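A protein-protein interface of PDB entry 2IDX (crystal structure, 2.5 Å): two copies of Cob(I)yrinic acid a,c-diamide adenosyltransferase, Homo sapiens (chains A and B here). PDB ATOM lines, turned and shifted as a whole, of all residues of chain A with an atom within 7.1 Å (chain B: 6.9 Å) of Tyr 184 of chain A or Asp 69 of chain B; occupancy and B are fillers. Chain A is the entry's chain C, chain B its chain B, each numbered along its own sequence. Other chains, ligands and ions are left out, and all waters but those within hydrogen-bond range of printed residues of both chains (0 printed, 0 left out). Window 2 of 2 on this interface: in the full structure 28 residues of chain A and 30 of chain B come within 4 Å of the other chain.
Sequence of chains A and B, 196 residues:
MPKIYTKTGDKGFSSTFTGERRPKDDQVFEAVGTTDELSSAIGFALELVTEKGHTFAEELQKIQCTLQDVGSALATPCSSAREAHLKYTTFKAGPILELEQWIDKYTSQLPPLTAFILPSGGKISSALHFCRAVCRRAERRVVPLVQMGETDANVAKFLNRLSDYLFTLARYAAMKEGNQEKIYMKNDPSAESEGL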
ATOM      1  N   ALA A 115     -22.747  -8.394 -28.107  1.00  0.00           N
ATOM      2  CA  ALA A 115     -22.518  -6.961 -28.167  1.00  0.00           C
ATOM      3  C   ALA A 115     -23.833  -6.201 -28.363  1.00  0.00           C
ATOM      4  O   ALA A 115     -24.879  -6.797 -28.642  1.00  0.00           O
ATOM      5  CB  ALA A 115     -21.502  -6.617 -29.263  1.00  0.00           C
ATOM      6  N   PHE A 116     -23.766  -4.889 -28.166  1.00  0.00           N
ATOM      7  CA  PHE A 116     -24.902  -4.029 -28.384  1.00  0.00           C
ATOM      8  C   PHE A 116     -25.127  -3.809 -29.876  1.00  0.00           C
ATOM      9  O   PHE A 116     -24.240  -3.370 -30.617  1.00  0.00           O
ATOM     10  CB  PHE A 116     -24.694  -2.687 -27.710  1.00  0.00           C
ATOM     11  CG  PHE A 116     -24.919  -2.696 -26.234  1.00  0.00           C
ATOM     12  CD1 PHE A 116     -23.840  -2.568 -25.353  1.00  0.00           C
ATOM     13  CD2 PHE A 116     -26.218  -2.785 -25.712  1.00  0.00           C
ATOM     14  CE1 PHE A 116     -24.046  -2.544 -23.948  1.00  0.00           C
ATOM     15  CE2 PHE A 116     -26.436  -2.771 -24.320  1.00  0.00           C
ATOM     16  CZ  PHE A 116     -25.343  -2.650 -23.438  1.00  0.00           C
ATOM     17  N   ILE A 117     -26.336  -4.130 -30.299  1.00  0.00           N
ATOM     18  CA  ILE A 117     -26.775  -3.941 -31.651  1.00  0.00           C
ATOM     19  C   ILE A 117     -27.395  -2.553 -31.773  1.00  0.00           C
ATOM     20  O   ILE A 117     -28.307  -2.195 -31.031  1.00  0.00           O
ATOM     21  CB  ILE A 117     -27.799  -5.019 -31.997  1.00  0.00           C
ATOM     22  CG1 ILE A 117     -27.098  -6.383 -32.088  1.00  0.00           C
ATOM     23  CG2 ILE A 117     -28.510  -4.683 -33.275  1.00  0.00           C
ATOM     24  CD1 ILE A 117     -27.966  -7.514 -32.586  1.00  0.00           C
ATOM     25  N   LEU A 118     -26.881  -1.763 -32.703  1.00  0.00           N
ATOM     26  CA  LEU A 118     -27.559  -0.543 -33.119  1.00  0.00           C
ATOM     27  C   LEU A 118     -28.767  -0.864 -34.011  1.00  0.00           C
ATOM     28  O   LEU A 118     -28.743  -1.858 -34.744  1.00  0.00           O
ATOM     29  CB  LEU A 118     -26.590   0.353 -33.891  1.00  0.00           C
ATOM     30  CG  LEU A 118     -25.279   0.655 -33.165  1.00  0.00           C
ATOM     31  CD1 LEU A 118     -24.296   1.387 -34.086  1.00  0.00           C
ATOM     32  CD2 LEU A 118     -25.540   1.426 -31.882  1.00  0.00           C
ATOM     33  N   LYS A 182     -25.324  -3.159 -37.352  1.00  0.00           N
ATOM     34  CA  LYS A 182     -24.195  -2.424 -36.836  1.00  0.00           C
ATOM     35  C   LYS A 182     -24.040  -2.704 -35.351  1.00  0.00           C
ATOM     36  O   LYS A 182     -25.004  -3.042 -34.667  1.00  0.00           O
ATOM     37  CB  LYS A 182     -24.391  -0.934 -37.100  1.00  0.00           C
ATOM     38  CG  LYS A 182     -24.932  -0.638 -38.481  1.00  0.00           C
ATOM     39  CD  LYS A 182     -23.913  -0.887 -39.591  1.00  0.00           C
ATOM     40  CE  LYS A 182     -24.583  -0.877 -40.955  1.00  0.00           C
ATOM     41  NZ  LYS A 182     -23.552  -0.959 -42.016  1.00  0.00           N
ATOM     42  N   ILE A 183     -22.821  -2.559 -34.862  1.00  0.00           N
ATOM     43  CA  ILE A 183     -22.478  -2.911 -33.487  1.00  0.00           C
ATOM     44  C   ILE A 183     -22.080  -1.635 -32.774  1.00  0.00           C
ATOM     45  O   ILE A 183     -21.452  -0.780 -33.377  1.00  0.00           O
ATOM     46  CB  ILE A 183     -21.303  -3.934 -33.483  1.00  0.00           C
ATOM     47  CG1 ILE A 183     -21.749  -5.256 -34.118  1.00  0.00           C
ATOM     48  CG2 ILE A 183     -20.738  -4.180 -32.083  1.00  0.00           C
ATOM     49  CD1 ILE A 183     -23.053  -5.836 -33.557  1.00  0.00           C
ATOM     50  N   TYR A 184     -22.450  -1.487 -31.507  1.00  0.00           N
ATOM     51  CA  TYR A 184     -22.001  -0.326 -30.744  1.00  0.00           C
ATOM     52  C   TYR A 184     -20.481  -0.222 -30.720  1.00  0.00           C
ATOM     53  O   TYR A 184     -19.791  -1.196 -30.471  1.00  0.00           O
ATOM     54  CB  TYR A 184     -22.552  -0.338 -29.323  1.00  0.00           C
ATOM     55  CG  TYR A 184     -21.906   0.691 -28.411  1.00  0.00           C
ATOM     56  CD1 TYR A 184     -22.298   2.034 -28.440  1.00  0.00           C
ATOM     57  CD2 TYR A 184     -20.886   0.325 -27.530  1.00  0.00           C
ATOM     58  CE1 TYR A 184     -21.698   2.965 -27.611  1.00  0.00           C
ATOM     59  CE2 TYR A 184     -20.295   1.242 -26.716  1.00  0.00           C
ATOM     60  CZ  TYR A 184     -20.705   2.555 -26.750  1.00  0.00           C
ATOM     61  OH  TYR A 184     -20.106   3.449 -25.920  1.00  0.00           O
ATOM     62  N   MET A 185     -19.973   0.972 -30.978  1.00  0.00           N
ATOM     63  CA  MET A 185     -18.541   1.174 -31.091  1.00  0.00           C
ATOM     64  C   MET A 185     -18.033   2.195 -30.072  1.00  0.00           C
ATOM     65  O   MET A 185     -18.752   2.614 -29.185  1.00  0.00           O
ATOM     66  CB  MET A 185     -18.202   1.609 -32.512  1.00  0.00           C
ATOM     67  CG  MET A 185     -16.919   1.042 -33.061  1.00  0.00           C
ATOM     68  SD  MET A 185     -16.158   2.201 -34.253  1.00  0.00           S
ATOM     69  CE  MET A 185     -15.091   3.189 -33.158  1.00  0.00           C
ATOM     70  N   LYS A 186     -16.783   2.616 -30.231  1.00  0.00           N
ATOM     71  CA  LYS A 186     -16.006   3.181 -29.127  1.00  0.00           C
ATOM     72  C   LYS A 186     -15.892   2.116 -28.013  1.00  0.00           C
ATOM     73  O   LYS A 186     -15.956   0.891 -28.268  1.00  0.00           O
ATOM     74  CB  LYS A 186     -16.609   4.499 -28.621  1.00  0.00           C
ATOM     75  CG  LYS A 186     -16.863   4.555 -27.097  1.00  0.00           C
ATOM     76  CD  LYS A 186     -15.571   4.704 -26.248  1.00  0.00           C
ATOM     77  CE  LYS A 186     -15.162   3.381 -25.547  1.00  0.00           C
ATOM     78  NZ  LYS A 186     -13.705   3.342 -25.140  1.00  0.00           N
ATOM     79  N   THR B  35     -34.730   8.655 -26.373  1.00  0.00           N
ATOM     80  CA  THR B  35     -33.412   8.559 -26.936  1.00  0.00           C
ATOM     81  C   THR B  35     -33.221   7.278 -27.786  1.00  0.00           C
ATOM     82  O   THR B  35     -32.623   7.348 -28.864  1.00  0.00           O
ATOM     83  CB  THR B  35     -32.314   8.717 -25.821  1.00  0.00           C
ATOM     84  OG1 THR B  35     -32.298  10.073 -25.345  1.00  0.00           O
ATOM     85  CG2 THR B  35     -30.958   8.406 -26.356  1.00  0.00           C
ATOM     86  N   ILE B  63     -23.472   8.808 -34.590  1.00  0.00           N
ATOM     87  CA  ILE B  63     -24.462   9.437 -33.746  1.00  0.00           C
ATOM     88  C   ILE B  63     -25.285   8.404 -32.965  1.00  0.00           C
ATOM     89  O   ILE B  63     -25.545   8.582 -31.773  1.00  0.00           O
ATOM     90  CB  ILE B  63     -25.344  10.368 -34.565  1.00  0.00           C
ATOM     91  CG1 ILE B  63     -24.564  11.670 -34.826  1.00  0.00           C
ATOM     92  CG2 ILE B  63     -26.669  10.598 -33.852  1.00  0.00           C
ATOM     93  CD1 ILE B  63     -24.969  12.416 -36.074  1.00  0.00           C
ATOM     94  N   GLN B  64     -25.666   7.308 -33.619  1.00  0.00           N
ATOM     95  CA  GLN B  64     -26.331   6.227 -32.915  1.00  0.00           C
ATOM     96  C   GLN B  64     -25.482   5.728 -31.764  1.00  0.00           C
ATOM     97  O   GLN B  64     -26.033   5.365 -30.724  1.00  0.00           O
ATOM     98  CB  GLN B  64     -26.643   5.067 -33.836  1.00  0.00           C
ATOM     99  CG  GLN B  64     -27.689   5.396 -34.848  1.00  0.00           C
ATOM    100  CD  GLN B  64     -27.974   4.214 -35.710  1.00  0.00           C
ATOM    101  OE1 GLN B  64     -27.099   3.743 -36.443  1.00  0.00           O
ATOM    102  NE2 GLN B  64     -29.189   3.690 -35.615  1.00  0.00           N
ATOM    103  N   CYS B  65     -24.161   5.710 -31.933  1.00  0.00           N
ATOM    104  CA  CYS B  65     -23.300   5.212 -30.862  1.00  0.00           C
ATOM    105  C   CYS B  65     -23.337   6.174 -29.717  1.00  0.00           C
ATOM    106  O   CYS B  65     -23.483   5.758 -28.570  1.00  0.00           O
ATOM    107  CB  CYS B  65     -21.860   4.932 -31.307  1.00  0.00           C
ATOM    108  SG  CYS B  65     -21.706   3.522 -32.447  1.00  0.00           S
ATOM    109  N   THR B  66     -23.221   7.468 -30.015  1.00  0.00           N
ATOM    110  CA  THR B  66     -23.340   8.483 -28.978  1.00  0.00           C
ATOM    111  C   THR B  66     -24.718   8.415 -28.286  1.00  0.00           C
ATOM    112  O   THR B  66     -24.817   8.626 -27.079  1.00  0.00           O
ATOM    113  CB  THR B  66     -23.068   9.896 -29.523  1.00  0.00           C
ATOM    114  OG1 THR B  66     -21.761   9.934 -30.097  1.00  0.00           O
ATOM    115  CG2 THR B  66     -23.095  10.902 -28.411  1.00  0.00           C
ATOM    116  N   LEU B  67     -25.763   8.094 -29.043  1.00  0.00           N
ATOM    117  CA  LEU B  67     -27.105   8.036 -28.452  1.00  0.00           C
ATOM    118  C   LEU B  67     -27.183   6.948 -27.396  1.00  0.00           C
ATOM    119  O   LEU B  67     -27.852   7.126 -26.365  1.00  0.00           O
ATOM    120  CB  LEU B  67     -28.230   7.925 -29.499  1.00  0.00           C
ATOM    121  CG  LEU B  67     -28.433   9.215 -30.314  1.00  0.00           C
ATOM    122  CD1 LEU B  67     -29.397   8.993 -31.452  1.00  0.00           C
ATOM    123  CD2 LEU B  67     -28.913  10.368 -29.440  1.00  0.00           C
ATOM    124  N   GLN B  68     -26.453   5.853 -27.610  1.00  0.00           N
ATOM    125  CA  GLN B  68     -26.339   4.875 -26.537  1.00  0.00           C
ATOM    126  C   GLN B  68     -25.671   5.493 -25.308  1.00  0.00           C
ATOM    127  O   GLN B  68     -26.195   5.373 -24.199  1.00  0.00           O
ATOM    128  CB  GLN B  68     -25.616   3.606 -26.957  1.00  0.00           C
ATOM    129  CG  GLN B  68     -25.427   2.673 -25.777  1.00  0.00           C
ATOM    130  CD  GLN B  68     -25.802   1.250 -26.090  1.00  0.00           C
ATOM    131  OE1 GLN B  68     -25.643   0.789 -27.220  1.00  0.00           O
ATOM    132  NE2 GLN B  68     -26.313   0.532 -25.084  1.00  0.00           N
ATOM    133  N   ASP B  69     -24.557   6.191 -25.505  1.00  0.00           N
ATOM    134  CA  ASP B  69     -23.924   6.865 -24.388  1.00  0.00           C
ATOM    135  C   ASP B  69     -24.851   7.860 -23.671  1.00  0.00           C
ATOM    136  O   ASP B  69     -24.814   7.961 -22.437  1.00  0.00           O
ATOM    137  CB  ASP B  69     -22.604   7.517 -24.810  1.00  0.00           C
ATOM    138  CG  ASP B  69     -21.586   6.495 -25.339  1.00  0.00           C
ATOM    139  OD1 ASP B  69     -20.731   6.871 -26.154  1.00  0.00           O
ATOM    140  OD2 ASP B  69     -21.631   5.318 -24.952  1.00  0.00           O
ATOM    141  N   VAL B  70     -25.659   8.597 -24.437  1.00  0.00           N
ATOM    142  CA  VAL B  70     -26.670   9.495 -23.877  1.00  0.00           C
ATOM    143  C   VAL B  70     -27.689   8.705 -23.039  1.00  0.00           C
ATOM    144  O   VAL B  70     -28.018   9.091 -21.927  1.00  0.00           O
ATOM    145  CB  VAL B  70     -27.411  10.250 -24.982  1.00  0.00           C
ATOM    146  CG1 VAL B  70     -28.564  11.007 -24.425  1.00  0.00           C
ATOM    147  CG2 VAL B  70     -26.466  11.188 -25.681  1.00  0.00           C
ATOM    148  N   GLY B  71     -28.172   7.599 -23.591  1.00  0.00           N
ATOM    149  CA  GLY B  71     -28.980   6.659 -22.831  1.00  0.00           C
ATOM    150  C   GLY B  71     -28.375   6.281 -21.486  1.00  0.00           C
ATOM    151  O   GLY B  71     -29.051   6.358 -20.463  1.00  0.00           O
ATOM    152  N   SER B  72     -27.103   5.905 -21.463  1.00  0.00           N
ATOM    153  CA  SER B  72     -26.493   5.422 -20.244  1.00  0.00           C
ATOM    154  C   SER B  72     -26.405   6.526 -19.247  1.00  0.00           C
ATOM    155  O   SER B  72     -26.630   6.317 -18.046  1.00  0.00           O
ATOM    156  CB  SER B  72     -25.081   4.930 -20.501  1.00  0.00           C
ATOM    157  OG  SER B  72     -25.133   3.821 -21.363  1.00  0.00           O
ATOM    158  N   ALA B  73     -26.024   7.698 -19.734  1.00  0.00           N
ATOM    159  CA  ALA B  73     -25.816   8.816 -18.863  1.00  0.00           C
ATOM    160  C   ALA B  73     -27.130   9.139 -18.157  1.00  0.00           C
ATOM    161  O   ALA B  73     -27.144   9.344 -16.942  1.00  0.00           O
ATOM    162  CB  ALA B  73     -25.312   9.999 -19.666  1.00  0.00           C
ATOM    163  N   LEU B  74     -28.223   9.153 -18.929  1.00  0.00           N
ATOM    164  CA  LEU B  74     -29.564   9.414 -18.427  1.00  0.00           C
ATOM    165  C   LEU B  74     -30.015   8.323 -17.470  1.00  0.00           C
ATOM    166  O   LEU B  74     -30.713   8.609 -16.517  1.00  0.00           O
ATOM    167  CB  LEU B  74     -30.564   9.550 -19.579  1.00  0.00           C
ATOM    168  CG  LEU B  74     -30.366  10.689 -20.586  1.00  0.00           C
ATOM    169  CD1 LEU B  74     -31.286  10.531 -21.797  1.00  0.00           C
ATOM    170  CD2 LEU B  74     -30.546  12.057 -19.936  1.00  0.00           C
ATOM    171  N   ALA B  75     -29.593   7.082 -17.707  1.00  0.00           N
ATOM    172  CA  ALA B  75     -29.953   5.970 -16.823  1.00  0.00           C
ATOM    173  C   ALA B  75     -29.176   6.005 -15.513  1.00  0.00           C
ATOM    174  O   ALA B  75     -29.371   5.159 -14.636  1.00  0.00           O
ATOM    175  CB  ALA B  75     -29.736   4.651 -17.513  1.00  0.00           C
ATOM    176  N   PHE B  91     -20.928  13.877 -18.836  1.00  0.00           N
ATOM    177  CA  PHE B  91     -20.959  13.735 -20.280  1.00  0.00           C
ATOM    178  C   PHE B  91     -19.987  14.732 -20.920  1.00  0.00           C
ATOM    179  O   PHE B  91     -20.184  15.944 -20.826  1.00  0.00           O
ATOM    180  CB  PHE B  91     -22.387  13.949 -20.778  1.00  0.00           C
ATOM    181  CG  PHE B  91     -22.610  13.510 -22.190  1.00  0.00           C
ATOM    182  CD1 PHE B  91     -22.838  12.180 -22.487  1.00  0.00           C
ATOM    183  CD2 PHE B  91     -22.598  14.430 -23.223  1.00  0.00           C
ATOM    184  CE1 PHE B  91     -23.035  11.772 -23.787  1.00  0.00           C
ATOM    185  CE2 PHE B  91     -22.791  14.021 -24.530  1.00  0.00           C
ATOM    186  CZ  PHE B  91     -23.008  12.694 -24.813  1.00  0.00           C
ATOM    187  N   PRO B  95     -18.564  14.929 -28.415  1.00  0.00           N
ATOM    188  CA  PRO B  95     -19.453  14.626 -29.545  1.00  0.00           C
ATOM    189  C   PRO B  95     -20.286  15.827 -29.985  1.00  0.00           C
ATOM    190  O   PRO B  95     -20.699  15.890 -31.144  1.00  0.00           O
ATOM    191  CB  PRO B  95     -20.338  13.484 -29.019  1.00  0.00           C
ATOM    192  CG  PRO B  95     -19.734  13.072 -27.717  1.00  0.00           C
ATOM    193  CD  PRO B  95     -18.990  14.249 -27.185  1.00  0.00           C
ATOM    194  N   VAL B 155     -25.695  16.872 -21.939  1.00  0.00           N
ATOM    195  CA  VAL B 155     -26.476  15.809 -22.560  1.00  0.00           C
ATOM    196  C   VAL B 155     -27.589  16.491 -23.323  1.00  0.00           C
ATOM    197  O   VAL B 155     -27.870  16.124 -24.469  1.00  0.00           O
ATOM    198  CB  VAL B 155     -27.060  14.805 -21.513  1.00  0.00           C
ATOM    199  CG1 VAL B 155     -28.212  13.963 -22.117  1.00  0.00           C
ATOM    200  CG2 VAL B 155     -25.963  13.910 -20.929  1.00  0.00           C
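CD2 of Phe 116 of chain A touches NE2 of Gln 68 of chain B (3.4 Å). CD1 of Leu 118 of chain A touches SG of Cys 65 of chain B, at 3.7 Å. CE1 of Tyr 184 of chain A touches O of Cys 65 of chain B (3.5 Å). Gln 68 of chain B touches Tyr 184 of chain A.
The backbone carbonyl oxygen of Gln 68 of chain B is in hydrogen-bond range of the side-chain hydroxyl of Ser 72 of chain B (3.4 Å). O of Phe 116 of chain A sits at hydrogen-bond distance from N of Tyr 184 of chain A (2.7 Å). O of Lys 182 of chain A lies within hydrogen-bond range of N of Leu 118 of chain A.
The side-chain sulfur of Cys 65 of chain B is in hydrogen-bond range of the backbone NH of Met 185 of chain A (3.4 Å). The side-chain carboxylate (OD2) of Asp 69 of chain B lies within hydrogen-bond range of the side-chain hydroxyl (OH) of Tyr 184 of chain A (2.6 Å).
No position is printed for both chains. Of the 6 pairs that touch across the chains among the printed residues, none has its exchanged pair printed and touching as well.
Along chain A the printed residues that touch a printed residue of chain B span positions 116 to 185. Among the printed residues, no Asp or Glu carboxylate lies within 4 Å of a Lys or Arg side-chain nitrogen of the other chain.
Printed residues of chain B within 4 Å of Phe 116 of chain A: Gln 68 (3.4 Å). Ile 117 of chain A touches none of the printed residues of chain B. Printed residues of chain B within 4 Å of Leu 118 of chain A: Cys 65. Of chain B, only Cys 65 (3.5 Å), Gln 68 (3.8 Å) and Asp 69 (2.6 Å) come within 4 Å of Tyr 184 of chain A. Of the printed residues of chain B, Met 185 of chain A touches Cys 65. Of the printed residues of chain A, Cys 65 of chain B touches Leu 118, Tyr 184 and Met 185. Printed residues of chain A within 4 Å of Gln 68 of chain B: Phe 116 and Tyr 184. Printed residues of chain A within 4 Å of Asp 69 of chain B: Tyr 184 (2.6 Å). The nearest residue of chain B that does not touch Tyr 184 of chain A is Thr 66 of chain B (5.3 Å).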
